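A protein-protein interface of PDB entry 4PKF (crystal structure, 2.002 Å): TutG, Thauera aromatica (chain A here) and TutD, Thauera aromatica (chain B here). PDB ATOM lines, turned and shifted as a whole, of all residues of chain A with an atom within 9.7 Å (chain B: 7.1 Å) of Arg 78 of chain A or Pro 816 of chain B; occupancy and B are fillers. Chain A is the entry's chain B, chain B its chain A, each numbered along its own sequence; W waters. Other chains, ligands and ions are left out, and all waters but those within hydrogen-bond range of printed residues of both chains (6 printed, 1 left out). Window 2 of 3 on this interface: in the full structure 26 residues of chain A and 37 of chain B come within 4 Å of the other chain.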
ATOM      1  N   ARG A  48      45.862 -15.247  17.977  1.00  0.00           N
ATOM      2  CA  ARG A  48      45.148 -15.844  19.094  1.00  0.00           C
ATOM      3  C   ARG A  48      46.064 -16.147  20.270  1.00  0.00           C
ATOM      4  O   ARG A  48      47.047 -16.855  20.128  1.00  0.00           O
ATOM      5  CB  ARG A  48      44.421 -17.078  18.619  1.00  0.00           C
ATOM      6  CG  ARG A  48      43.138 -16.638  17.934  1.00  0.00           C
ATOM      7  CD  ARG A  48      42.736 -17.616  16.943  1.00  0.00           C
ATOM      8  NE  ARG A  48      41.687 -17.119  16.038  1.00  0.00           N
ATOM      9  CZ  ARG A  48      40.428 -17.486  16.102  1.00  0.00           C
ATOM     10  NH1 ARG A  48      39.588 -17.037  15.189  1.00  0.00           N
ATOM     11  NH2 ARG A  48      40.001 -18.324  17.067  1.00  0.00           N
ATOM     12  N   VAL A  54      41.261 -13.108  21.304  1.00  0.00           N
ATOM     13  CA  VAL A  54      41.329 -13.116  19.848  1.00  0.00           C
ATOM     14  C   VAL A  54      41.592 -11.671  19.447  1.00  0.00           C
ATOM     15  O   VAL A  54      40.668 -10.844  19.322  1.00  0.00           O
ATOM     16  CB  VAL A  54      40.040 -13.661  19.199  1.00  0.00           C
ATOM     17  CG1 VAL A  54      40.149 -13.603  17.677  1.00  0.00           C
ATOM     18  CG2 VAL A  54      39.775 -15.128  19.682  1.00  0.00           C
ATOM     19  N   LYS A  74      37.915 -21.976   5.779  1.00  0.00           N
ATOM     20  CA  LYS A  74      36.863 -21.280   6.517  1.00  0.00           C
ATOM     21  C   LYS A  74      36.667 -21.937   7.874  1.00  0.00           C
ATOM     22  O   LYS A  74      36.497 -23.144   7.950  1.00  0.00           O
ATOM     23  CB  LYS A  74      35.545 -21.292   5.722  1.00  0.00           C
ATOM     24  CG  LYS A  74      34.498 -20.282   6.193  1.00  0.00           C
ATOM     25  CD  LYS A  74      33.246 -20.337   5.294  1.00  0.00           C
ATOM     26  CE  LYS A  74      32.345 -19.131   5.509  1.00  0.00           C
ATOM     27  NZ  LYS A  74      31.732 -19.216   6.861  1.00  0.00           N
ATOM     28  N   LEU A  75      36.721 -21.140   8.937  1.00  0.00           N
ATOM     29  CA  LEU A  75      36.515 -21.635  10.295  1.00  0.00           C
ATOM     30  C   LEU A  75      35.026 -21.740  10.553  1.00  0.00           C
ATOM     31  O   LEU A  75      34.264 -20.983   9.958  1.00  0.00           O
ATOM     32  CB  LEU A  75      37.171 -20.698  11.316  1.00  0.00           C
ATOM     33  CG  LEU A  75      38.689 -20.568  11.228  1.00  0.00           C
ATOM     34  CD1 LEU A  75      39.190 -19.560  12.254  1.00  0.00           C
ATOM     35  CD2 LEU A  75      39.342 -21.946  11.441  1.00  0.00           C
ATOM     36  N   SER A  76      34.586 -22.653  11.422  1.00  0.00           N
ATOM     37  CA  SER A  76      33.147 -22.638  11.742  1.00  0.00           C
ATOM     38  C   SER A  76      32.904 -21.497  12.711  1.00  0.00           C
ATOM     39  O   SER A  76      33.860 -20.889  13.208  1.00  0.00           O
ATOM     40  CB  SER A  76      32.655 -23.977  12.319  1.00  0.00           C
ATOM     41  OG  SER A  76      32.884 -24.097  13.714  1.00  0.00           O
ATOM     42  N   PHE A  77      31.637 -21.205  12.975  1.00  0.00           N
ATOM     43  CA  PHE A  77      31.274 -20.149  13.900  1.00  0.00           C
ATOM     44  C   PHE A  77      31.913 -20.409  15.250  1.00  0.00           C
ATOM     45  O   PHE A  77      32.237 -19.472  15.982  1.00  0.00           O
ATOM     46  CB  PHE A  77      29.736 -20.038  14.047  1.00  0.00           C
ATOM     47  CG  PHE A  77      29.120 -21.140  14.852  1.00  0.00           C
ATOM     48  CD1 PHE A  77      28.740 -22.323  14.252  1.00  0.00           C
ATOM     49  CD2 PHE A  77      28.908 -20.988  16.209  1.00  0.00           C
ATOM     50  CE1 PHE A  77      28.157 -23.337  14.985  1.00  0.00           C
ATOM     51  CE2 PHE A  77      28.316 -22.017  16.958  1.00  0.00           C
ATOM     52  CZ  PHE A  77      27.946 -23.190  16.334  1.00  0.00           C
ATOM     53  N   ARG A  78      32.077 -21.687  15.595  1.00  0.00           N
ATOM     54  CA  ARG A  78      32.609 -22.044  16.918  1.00  0.00           C
ATOM     55  C   ARG A  78      33.973 -21.413  17.209  1.00  0.00           C
ATOM     56  O   ARG A  78      34.321 -21.144  18.369  1.00  0.00           O
ATOM     57  CB  ARG A  78      32.725 -23.574  17.051  1.00  0.00           C
ATOM     58  CG  ARG A  78      31.391 -24.339  16.947  1.00  0.00           C
ATOM     59  CD  ARG A  78      31.461 -25.766  17.614  1.00  0.00           C
ATOM     60  NE  ARG A  78      30.179 -26.437  17.418  1.00  0.00           N
ATOM     61  CZ  ARG A  78      29.112 -26.175  18.147  1.00  0.00           C
ATOM     62  NH1 ARG A  78      29.214 -25.294  19.134  1.00  0.00           N
ATOM     63  NH2 ARG A  78      27.953 -26.780  17.901  1.00  0.00           N
ATOM     64  N   ASP A  79      34.762 -21.214  16.161  1.00  0.00           N
ATOM     65  CA  ASP A  79      36.123 -20.727  16.324  1.00  0.00           C
ATOM     66  C   ASP A  79      36.291 -19.222  16.058  1.00  0.00           C
ATOM     67  O   ASP A  79      37.407 -18.718  16.037  1.00  0.00           O
ATOM     68  CB  ASP A  79      37.046 -21.515  15.410  1.00  0.00           C
ATOM     69  CG  ASP A  79      37.146 -22.984  15.837  1.00  0.00           C
ATOM     70  OD1 ASP A  79      37.371 -23.238  17.036  1.00  0.00           O
ATOM     71  OD2 ASP A  79      36.956 -23.864  14.983  1.00  0.00           O
ATOM     72  N   HIS A  80      35.182 -18.523  15.861  1.00  0.00           N
ATOM     73  CA  HIS A  80      35.223 -17.071  15.642  1.00  0.00           C
ATOM     74  C   HIS A  80      34.654 -16.360  16.867  1.00  0.00           C
ATOM     75  O   HIS A  80      34.192 -17.007  17.797  1.00  0.00           O
ATOM     76  CB  HIS A  80      34.436 -16.687  14.380  1.00  0.00           C
ATOM     77  CG  HIS A  80      35.241 -16.730  13.122  1.00  0.00           C
ATOM     78  ND1 HIS A  80      36.341 -15.917  12.910  1.00  0.00           N
ATOM     79  CD2 HIS A  80      35.104 -17.479  11.998  1.00  0.00           C
ATOM     80  CE1 HIS A  80      36.845 -16.165  11.711  1.00  0.00           C
ATOM     81  NE2 HIS A  80      36.109 -17.103  11.132  1.00  0.00           N
ATOM     82  N   VAL A  81      34.716 -15.033  16.889  1.00  0.00           N
ATOM     83  CA  VAL A  81      34.125 -14.274  17.982  1.00  0.00           C
ATOM     84  C   VAL A  81      32.650 -13.953  17.630  1.00  0.00           C
ATOM     85  O   VAL A  81      31.690 -14.269  18.362  1.00  0.00           O
ATOM     86  CB  VAL A  81      34.913 -12.964  18.257  1.00  0.00           C
ATOM     87  CG1 VAL A  81      34.257 -12.147  19.381  1.00  0.00           C
ATOM     88  CG2 VAL A  81      36.376 -13.283  18.573  1.00  0.00           C
ATOM     89  OXT VAL A  81      32.382 -13.371  16.568  1.00  0.00           O
ATOM     90  N   GLU B  36      18.721 -31.102  30.286  1.00  0.00           N
ATOM     91  CA  GLU B  36      18.161 -31.959  29.256  1.00  0.00           C
ATOM     92  C   GLU B  36      16.954 -32.708  29.820  1.00  0.00           C
ATOM     93  O   GLU B  36      16.260 -33.420  29.103  1.00  0.00           O
ATOM     94  CB  GLU B  36      19.219 -32.924  28.719  1.00  0.00           C
ATOM     95  CG  GLU B  36      20.464 -32.194  28.143  1.00  0.00           C
ATOM     96  CD  GLU B  36      20.103 -31.059  27.137  1.00  0.00           C
ATOM     97  OE1 GLU B  36      20.541 -29.890  27.373  1.00  0.00           O
ATOM     98  OE2 GLU B  36      19.414 -31.338  26.114  1.00  0.00           O
ATOM     99  N   SER B  59      25.521 -16.565  14.778  1.00  0.00           N
ATOM    100  CA  SER B  59      26.661 -16.246  15.645  1.00  0.00           C
ATOM    101  C   SER B  59      27.829 -15.888  14.749  1.00  0.00           C
ATOM    102  O   SER B  59      27.905 -16.360  13.621  1.00  0.00           O
ATOM    103  CB  SER B  59      27.078 -17.427  16.563  1.00  0.00           C
ATOM    104  OG  SER B  59      26.122 -17.669  17.587  1.00  0.00           O
ATOM    105  N   ALA B  60      28.735 -15.071  15.264  1.00  0.00           N
ATOM    106  CA  ALA B  60      29.975 -14.744  14.577  1.00  0.00           C
ATOM    107  C   ALA B  60      29.739 -14.132  13.181  1.00  0.00           C
ATOM    108  O   ALA B  60      30.616 -14.167  12.328  1.00  0.00           O
ATOM    109  CB  ALA B  60      30.844 -15.991  14.487  1.00  0.00           C
ATOM    110  N   ILE B  64      23.954 -20.325  11.880  1.00  0.00           N
ATOM    111  CA  ILE B  64      24.451 -21.608  12.362  1.00  0.00           C
ATOM    112  C   ILE B  64      24.167 -22.710  11.341  1.00  0.00           C
ATOM    113  O   ILE B  64      24.974 -23.609  11.155  1.00  0.00           O
ATOM    114  CB  ILE B  64      23.794 -22.014  13.714  1.00  0.00           C
ATOM    115  CG1 ILE B  64      24.099 -21.014  14.838  1.00  0.00           C
ATOM    116  CG2 ILE B  64      24.202 -23.420  14.116  1.00  0.00           C
ATOM    117  CD1 ILE B  64      25.495 -20.539  14.883  1.00  0.00           C
ATOM    118  N   ALA B 811      30.507 -29.811  29.549  1.00  0.00           N
ATOM    119  CA  ALA B 811      30.011 -30.987  28.845  1.00  0.00           C
ATOM    120  C   ALA B 811      29.414 -30.624  27.487  1.00  0.00           C
ATOM    121  O   ALA B 811      29.610 -31.336  26.510  1.00  0.00           O
ATOM    122  CB  ALA B 811      28.974 -31.726  29.710  1.00  0.00           C
ATOM    123  N   ALA B 812      28.693 -29.502  27.427  1.00  0.00           N
ATOM    124  CA  ALA B 812      28.079 -29.039  26.181  1.00  0.00           C
ATOM    125  C   ALA B 812      29.097 -28.521  25.179  1.00  0.00           C
ATOM    126  O   ALA B 812      28.831 -28.508  23.975  1.00  0.00           O
ATOM    127  CB  ALA B 812      27.023 -27.955  26.483  1.00  0.00           C
ATOM    128  N   GLN B 813      30.259 -28.076  25.659  1.00  0.00           N
ATOM    129  CA  GLN B 813      31.338 -27.759  24.748  1.00  0.00           C
ATOM    130  C   GLN B 813      31.936 -29.017  24.136  1.00  0.00           C
ATOM    131  O   GLN B 813      32.229 -29.043  22.926  1.00  0.00           O
ATOM    132  CB  GLN B 813      32.444 -26.947  25.448  1.00  0.00           C
ATOM    133  CG  GLN B 813      31.986 -25.544  25.872  1.00  0.00           C
ATOM    134  CD  GLN B 813      33.103 -24.711  26.473  1.00  0.00           C
ATOM    135  OE1 GLN B 813      33.856 -25.180  27.322  1.00  0.00           O
ATOM    136  NE2 GLN B 813      33.231 -23.468  26.008  1.00  0.00           N
ATOM    137  N   ARG B 814      32.142 -30.038  24.962  1.00  0.00           N
ATOM    138  CA  ARG B 814      32.723 -31.291  24.471  1.00  0.00           C
ATOM    139  C   ARG B 814      31.810 -32.023  23.497  1.00  0.00           C
ATOM    140  O   ARG B 814      32.269 -32.604  22.513  1.00  0.00           O
ATOM    141  CB  ARG B 814      33.032 -32.232  25.630  1.00  0.00           C
ATOM    142  CG  ARG B 814      34.151 -31.753  26.537  1.00  0.00           C
ATOM    143  CD  ARG B 814      34.646 -32.877  27.468  1.00  0.00           C
ATOM    144  NE  ARG B 814      33.592 -33.412  28.330  1.00  0.00           N
ATOM    145  CZ  ARG B 814      33.244 -32.870  29.496  1.00  0.00           C
ATOM    146  NH1 ARG B 814      33.854 -31.766  29.934  1.00  0.00           N
ATOM    147  NH2 ARG B 814      32.284 -33.424  30.221  1.00  0.00           N
ATOM    148  N   GLU B 815      30.514 -32.009  23.797  1.00  0.00           N
ATOM    149  CA  GLU B 815      29.552 -32.842  23.111  1.00  0.00           C
ATOM    150  C   GLU B 815      28.284 -32.043  22.870  1.00  0.00           C
ATOM    151  O   GLU B 815      27.256 -32.298  23.492  1.00  0.00           O
ATOM    152  CB  GLU B 815      29.213 -34.084  23.944  1.00  0.00           C
ATOM    153  CG  GLU B 815      30.408 -34.952  24.323  1.00  0.00           C
ATOM    154  CD  GLU B 815      29.937 -36.297  24.905  1.00  0.00           C
ATOM    155  OE1 GLU B 815      29.817 -37.264  24.125  1.00  0.00           O
ATOM    156  OE2 GLU B 815      29.627 -36.355  26.116  1.00  0.00           O
ATOM    157  N   PRO B 816      28.369 -31.046  21.986  1.00  0.00           N
ATOM    158  CA  PRO B 816      27.220 -30.148  21.785  1.00  0.00           C
ATOM    159  C   PRO B 816      25.957 -30.903  21.384  1.00  0.00           C
ATOM    160  O   PRO B 816      24.858 -30.463  21.738  1.00  0.00           O
ATOM    161  CB  PRO B 816      27.682 -29.219  20.664  1.00  0.00           C
ATOM    162  CG  PRO B 816      28.826 -29.959  19.958  1.00  0.00           C
ATOM    163  CD  PRO B 816      29.481 -30.781  21.059  1.00  0.00           C
ATOM    164  N   GLU B 817      26.099 -32.021  20.676  1.00  0.00           N
ATOM    165  CA  GLU B 817      24.907 -32.728  20.174  1.00  0.00           C
ATOM    166  C   GLU B 817      24.069 -33.367  21.302  1.00  0.00           C
ATOM    167  O   GLU B 817      22.917 -33.731  21.099  1.00  0.00           O
ATOM    168  CB  GLU B 817      25.321 -33.780  19.130  1.00  0.00           C
ATOM    169  CG  GLU B 817      26.045 -35.012  19.690  1.00  0.00           C
ATOM    170  CD  GLU B 817      27.507 -34.764  20.189  1.00  0.00           C
ATOM    171  OE1 GLU B 817      28.027 -35.659  20.913  1.00  0.00           O
ATOM    172  OE2 GLU B 817      28.132 -33.708  19.872  1.00  0.00           O
ATOM    173  N   LYS B 818      24.642 -33.474  22.497  1.00  0.00           N
ATOM    174  CA  LYS B 818      23.947 -34.032  23.648  1.00  0.00           C
ATOM    175  C   LYS B 818      23.350 -32.956  24.555  1.00  0.00           C
ATOM    176  O   LYS B 818      22.796 -33.271  25.605  1.00  0.00           O
ATOM    177  CB  LYS B 818      24.919 -34.918  24.466  1.00  0.00           C
ATOM    178  CG  LYS B 818      25.231 -36.237  23.773  1.00  0.00           C
ATOM    179  CD  LYS B 818      26.209 -37.122  24.549  1.00  0.00           C
ATOM    180  CE  LYS B 818      26.635 -38.315  23.699  1.00  0.00           C
ATOM    181  NZ  LYS B 818      27.588 -39.181  24.438  1.00  0.00           N
ATOM    182  N   HIS B 819      23.468 -31.682  24.161  1.00  0.00           N
ATOM    183  CA  HIS B 819      23.059 -30.598  25.042  1.00  0.00           C
ATOM    184  C   HIS B 819      22.224 -29.522  24.320  1.00  0.00           C
ATOM    185  O   HIS B 819      22.368 -28.333  24.586  1.00  0.00           O
ATOM    186  CB  HIS B 819      24.302 -29.984  25.699  1.00  0.00           C
ATOM    187  CG  HIS B 819      25.023 -30.947  26.587  1.00  0.00           C
ATOM    188  ND1 HIS B 819      24.680 -31.131  27.909  1.00  0.00           N
ATOM    189  CD2 HIS B 819      26.019 -31.828  26.324  1.00  0.00           C
ATOM    190  CE1 HIS B 819      25.447 -32.081  28.433  1.00  0.00           C
ATOM    191  NE2 HIS B 819      26.256 -32.527  27.490  1.00  0.00           N
ATOM    192  N   HIS B 820      21.321 -29.971  23.459  1.00  0.00           N
ATOM    193  CA  HIS B 820      20.522 -29.070  22.639  1.00  0.00           C
ATOM    194  C   HIS B 820      19.595 -28.179  23.470  1.00  0.00           C
ATOM    195  O   HIS B 820      19.300 -27.049  23.058  1.00  0.00           O
ATOM    196  CB  HIS B 820      19.710 -29.873  21.616  1.00  0.00           C
ATOM    197  CG  HIS B 820      19.140 -29.044  20.505  1.00  0.00           C
ATOM    198  ND1 HIS B 820      17.784 -28.824  20.355  1.00  0.00           N
ATOM    199  CD2 HIS B 820      19.742 -28.376  19.486  1.00  0.00           C
ATOM    200  CE1 HIS B 820      17.572 -28.074  19.285  1.00  0.00           C
ATOM    201  NE2 HIS B 820      18.742 -27.784  18.741  1.00  0.00           N
ATOM    202  N   ASP B 821      19.135 -28.652  24.623  1.00  0.00           N
ATOM    203  CA  ASP B 821      18.184 -27.846  25.381  1.00  0.00           C
ATOM    204  C   ASP B 821      18.810 -27.007  26.469  1.00  0.00           C
ATOM    205  O   ASP B 821      18.097 -26.476  27.316  1.00  0.00           O
ATOM    206  CB  ASP B 821      17.083 -28.727  26.009  1.00  0.00           C
ATOM    207  CG  ASP B 821      15.669 -28.099  25.876  1.00  0.00           C
ATOM    208  OD1 ASP B 821      15.295 -27.598  24.787  1.00  0.00           O
ATOM    209  OD2 ASP B 821      14.926 -28.095  26.870  1.00  0.00           O
ATOM    210  N   PHE B 833      23.035 -22.469  24.283  1.00  0.00           N
ATOM    211  CA  PHE B 833      24.448 -22.444  24.618  1.00  0.00           C
ATOM    212  C   PHE B 833      25.331 -23.029  23.515  1.00  0.00           C
ATOM    213  O   PHE B 833      26.387 -22.461  23.205  1.00  0.00           O
ATOM    214  CB  PHE B 833      24.705 -23.197  25.927  1.00  0.00           C
ATOM    215  CG  PHE B 833      26.156 -23.216  26.340  1.00  0.00           C
ATOM    216  CD1 PHE B 833      26.698 -22.158  27.056  1.00  0.00           C
ATOM    217  CD2 PHE B 833      26.977 -24.299  26.019  1.00  0.00           C
ATOM    218  CE1 PHE B 833      28.038 -22.170  27.443  1.00  0.00           C
ATOM    219  CE2 PHE B 833      28.322 -24.332  26.397  1.00  0.00           C
ATOM    220  CZ  PHE B 833      28.861 -23.265  27.101  1.00  0.00           C
ATOM    221  N   VAL B 834      24.916 -24.165  22.939  1.00  0.00           N
ATOM    222  CA  VAL B 834      25.734 -24.829  21.911  1.00  0.00           C
ATOM    223  C   VAL B 834      25.771 -24.019  20.590  1.00  0.00           C
ATOM    224  O   VAL B 834      26.550 -24.308  19.675  1.00  0.00           O
ATOM    225  CB  VAL B 834      25.223 -26.286  21.610  1.00  0.00           C
ATOM    226  CG1 VAL B 834      25.406 -27.238  22.829  1.00  0.00           C
ATOM    227  CG2 VAL B 834      23.794 -26.250  21.134  1.00  0.00           C
ATOM    228  N   ASP B 835      24.946 -22.981  20.494  1.00  0.00           N
ATOM    229  CA  ASP B 835      24.980 -22.134  19.312  1.00  0.00           C
ATOM    230  C   ASP B 835      25.835 -20.877  19.519  1.00  0.00           C
ATOM    231  O   ASP B 835      25.923 -20.041  18.617  1.00  0.00           O
ATOM    232  CB  ASP B 835      23.577 -21.754  18.898  1.00  0.00           C
ATOM    233  CG  ASP B 835      22.797 -22.931  18.337  1.00  0.00           C
ATOM    234  OD1 ASP B 835      23.424 -23.979  18.065  1.00  0.00           O
ATOM    235  OD2 ASP B 835      21.557 -22.800  18.148  1.00  0.00           O
ATOM    236  N   ILE B 836      26.457 -20.758  20.689  1.00  0.00           N
ATOM    237  CA  ILE B 836      27.389 -19.644  20.967  1.00  0.00           C
ATOM    238  C   ILE B 836      28.820 -20.073  20.618  1.00  0.00           C
ATOM    239  O   ILE B 836      29.187 -21.213  20.903  1.00  0.00           O
ATOM    240  CB  ILE B 836      27.322 -19.213  22.459  1.00  0.00           C
ATOM    241  CG1 ILE B 836      25.871 -18.870  22.875  1.00  0.00           C
ATOM    242  CG2 ILE B 836      28.291 -17.991  22.730  1.00  0.00           C
ATOM    243  CD1 ILE B 836      25.713 -18.662  24.429  1.00  0.00           C
ATOM    244  N   PRO B 837      29.632 -19.179  20.005  1.00  0.00           N
ATOM    245  CA  PRO B 837      31.017 -19.587  19.740  1.00  0.00           C
ATOM    246  C   PRO B 837      31.776 -19.838  21.042  1.00  0.00           C
ATOM    247  O   PRO B 837      31.392 -19.336  22.097  1.00  0.00           O
ATOM    248  CB  PRO B 837      31.631 -18.386  19.009  1.00  0.00           C
ATOM    249  CG  PRO B 837      30.442 -17.599  18.493  1.00  0.00           C
ATOM    250  CD  PRO B 837      29.348 -17.829  19.489  1.00  0.00           C
ATOM    251  N   THR B 838      32.849 -20.616  20.952  1.00  0.00           N
ATOM    252  CA  THR B 838      33.579 -21.019  22.141  1.00  0.00           C
ATOM    253  C   THR B 838      34.044 -19.810  22.952  1.00  0.00           C
ATOM    254  O   THR B 838      33.995 -19.812  24.187  1.00  0.00           O
ATOM    255  CB  THR B 838      34.795 -21.883  21.741  1.00  0.00           C
ATOM    256  OG1 THR B 838      34.314 -23.021  21.005  1.00  0.00           O
ATOM    257  CG2 THR B 838      35.583 -22.355  23.008  1.00  0.00           C
ATOM    258  N   TYR B 839      34.494 -18.782  22.241  1.00  0.00           N
ATOM    259  CA  TYR B 839      34.974 -17.557  22.892  1.00  0.00           C
ATOM    260  C   TYR B 839      33.900 -16.992  23.815  1.00  0.00           C
ATOM    261  O   TYR B 839      34.163 -16.730  24.993  1.00  0.00           O
ATOM    262  CB  TYR B 839      35.383 -16.548  21.827  1.00  0.00           C
ATOM    263  CG  TYR B 839      35.873 -15.210  22.289  1.00  0.00           C
ATOM    264  CD1 TYR B 839      34.974 -14.197  22.612  1.00  0.00           C
ATOM    265  CD2 TYR B 839      37.233 -14.911  22.317  1.00  0.00           C
ATOM    266  CE1 TYR B 839      35.417 -12.910  22.994  1.00  0.00           C
ATOM    267  CE2 TYR B 839      37.695 -13.634  22.708  1.00  0.00           C
ATOM    268  CZ  TYR B 839      36.766 -12.631  23.035  1.00  0.00           C
ATOM    269  OH  TYR B 839      37.177 -11.347  23.417  1.00  0.00           O
ATOM    270  N   GLY B 840      32.681 -16.859  23.293  1.00  0.00           N
ATOM    271  CA  GLY B 840      31.574 -16.346  24.077  1.00  0.00           C
ATOM    272  C   GLY B 840      31.157 -17.308  25.170  1.00  0.00           C
ATOM    273  O   GLY B 840      30.796 -16.890  26.273  1.00  0.00           O
ATOM    274  N   GLN B 841      31.184 -18.608  24.871  1.00  0.00           N
ATOM    275  CA  GLN B 841      30.810 -19.608  25.894  1.00  0.00           C
ATOM    276  C   GLN B 841      31.733 -19.459  27.099  1.00  0.00           C
ATOM    277  O   GLN B 841      31.290 -19.478  28.245  1.00  0.00           O
ATOM    278  CB  GLN B 841      30.901 -21.032  25.347  1.00  0.00           C
ATOM    279  CG  GLN B 841      29.897 -21.413  24.258  1.00  0.00           C
ATOM    280  CD  GLN B 841      30.213 -22.810  23.711  1.00  0.00           C
ATOM    281  OE1 GLN B 841      31.373 -23.223  23.718  1.00  0.00           O
ATOM    282  NE2 GLN B 841      29.199 -23.526  23.236  1.00  0.00           N
HETATM  283  O   HOH W   1      29.139 -26.270  22.207  1.00  0.00           O
HETATM  284  O   HOH W   2      30.849 -23.222  20.024  1.00  0.00           O
HETATM  285  O   HOH W   3      29.075 -14.031  17.837  1.00  0.00           O
HETATM  286  O   HOH W   4      35.905 -24.214  19.232  1.00  0.00           O
HETATM  287  O   HOH W   5      35.263 -18.838  19.386  1.00  0.00           O
HETATM  288  O   HOH W   6      31.528 -15.131  20.779  1.00  0.00           O
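The guanidinium group (NH1) of Arg 78 of chain A sits at hydrogen-bond distance from the backbone carbonyl oxygen (O) of Val 834 of chain B, at 2.9 Å.
N of Thr 838 of chain B sits at hydrogen-bond distance from O of Arg 78 of chain A (3.0 Å).
The backbone NH of Arg 78 of chain A lies close to the side-chain hydroxyl of Ser 76 of chain A, at 3.2 Å.
OG of Ser 59 of chain B sits at hydrogen-bond distance from O of Asp 835 of chain B.
Among the printed residues, merely in contact across the chains: His 80 of chain A with Pro 837 of chain B, Phe 77 of chain A with Pro 837 of chain B, Val 81 of chain A with Ala 60 of chain B, Phe 77 of chain A with Asp 835 of chain B, Val 81 of chain A with Pro 837 of chain B, His 80 of chain A with Ala 60 of chain B, Val 54 of chain A with Tyr 839 of chain B, Phe 77 of chain A with Ile 64 of chain B, Arg 78 of chain A with Pro 816 of chain B, Phe 77 of chain A with Val 834 of chain B, Val 81 of chain A with Tyr 839 of chain B and Arg 78 of chain A with Pro 837 of chain B.
Of the 24 printed residues of chain B, 8 touch a printed residue of chain A.
Hydrophobic or aromatic side chains of chain B within 4 Å of the printed part of chain A: Ala 60, Ile 64, Pro 816, Pro 837 and Tyr 839.
Along chain B the printed residues that touch a printed residue of chain A span positions 60 to 839.
Of the 10 printed residues of chain A, 5 touch a printed residue of chain B.
Hydrophobic or aromatic side chains of chain A that line the printed part of chain B: Val 54, Phe 77, His 80 and Val 81.
Among the printed residues, 14 pairs touch across the chains.
Among the printed residues, no Asp or Glu carboxylate lies within 4 Å of a Lys or Arg side-chain nitrogen of the other chain.
Water W6 bridges the chain-end carboxylate (O) of Val 81 of chain A (2.6 Å) and the backbone NH (N) of Gly 840 of chain B (3.3 Å).
Water W5 lies within hydrogen-bond range of the backbone carbonyl oxygen of His 80 of chain A (2.7 Å), the backbone carbonyl oxygen of Arg 78 of chain A (2.7 Å), the backbone NH of Tyr 839 of chain B (3.0 Å) and the backbone NH of Thr 838 of chain B (3.4 Å).
Water W4 lies within hydrogen-bond range of OG1 of Thr 838 of chain B and OD1 of Asp 79 of chain A.
Water W3 lies within hydrogen-bond range of the chain-end carboxylate (O) of Val 81 of chain A (2.7 Å) and the backbone NH (N) of Ala 60 of chain B (2.8 Å).
Water W2 lies within hydrogen-bond range of O of Ile 836 of chain B (2.8 Å), NH1 of Arg 78 of chain A (2.8 Å) and N of Thr 838 of chain B (3.4 Å).
Water W1 lies within hydrogen-bond range of O of Ala 812 of chain B (2.9 Å), NE2 of Gln 841 of chain B (2.9 Å) and NH1 of Arg 78 of chain A (3.2 Å).
Arg 78 of chain A touches just these residues of chain B: Pro 816, Val 834, Pro 837 and Thr 838.
Of chain A, only Arg 78 comes within 4 Å of Pro 816 of chain B.
Printed residues of chain B within 4 Å of Val 81 of chain A: Ala 60 (3.4 Å), Pro 837 (3.6 Å) and Tyr 839 (3.9 Å).
Of the printed residues of chain A, Thr 838 of chain B touches Arg 78 (3.0 Å).
Of the printed residues of chain A, Tyr 839 of chain B touches Val 54 and Val 81.
Of the printed residues of chain B, His 80 of chain A touches Ala 60 (3.7 Å) and Pro 837 (3.2 Å).
Phe 833 of chain B touches none of the printed residues of chain A.
The nearest residue of chain A that does not touch Pro 816 of chain B is Phe 77 of chain A (7.4 Å).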
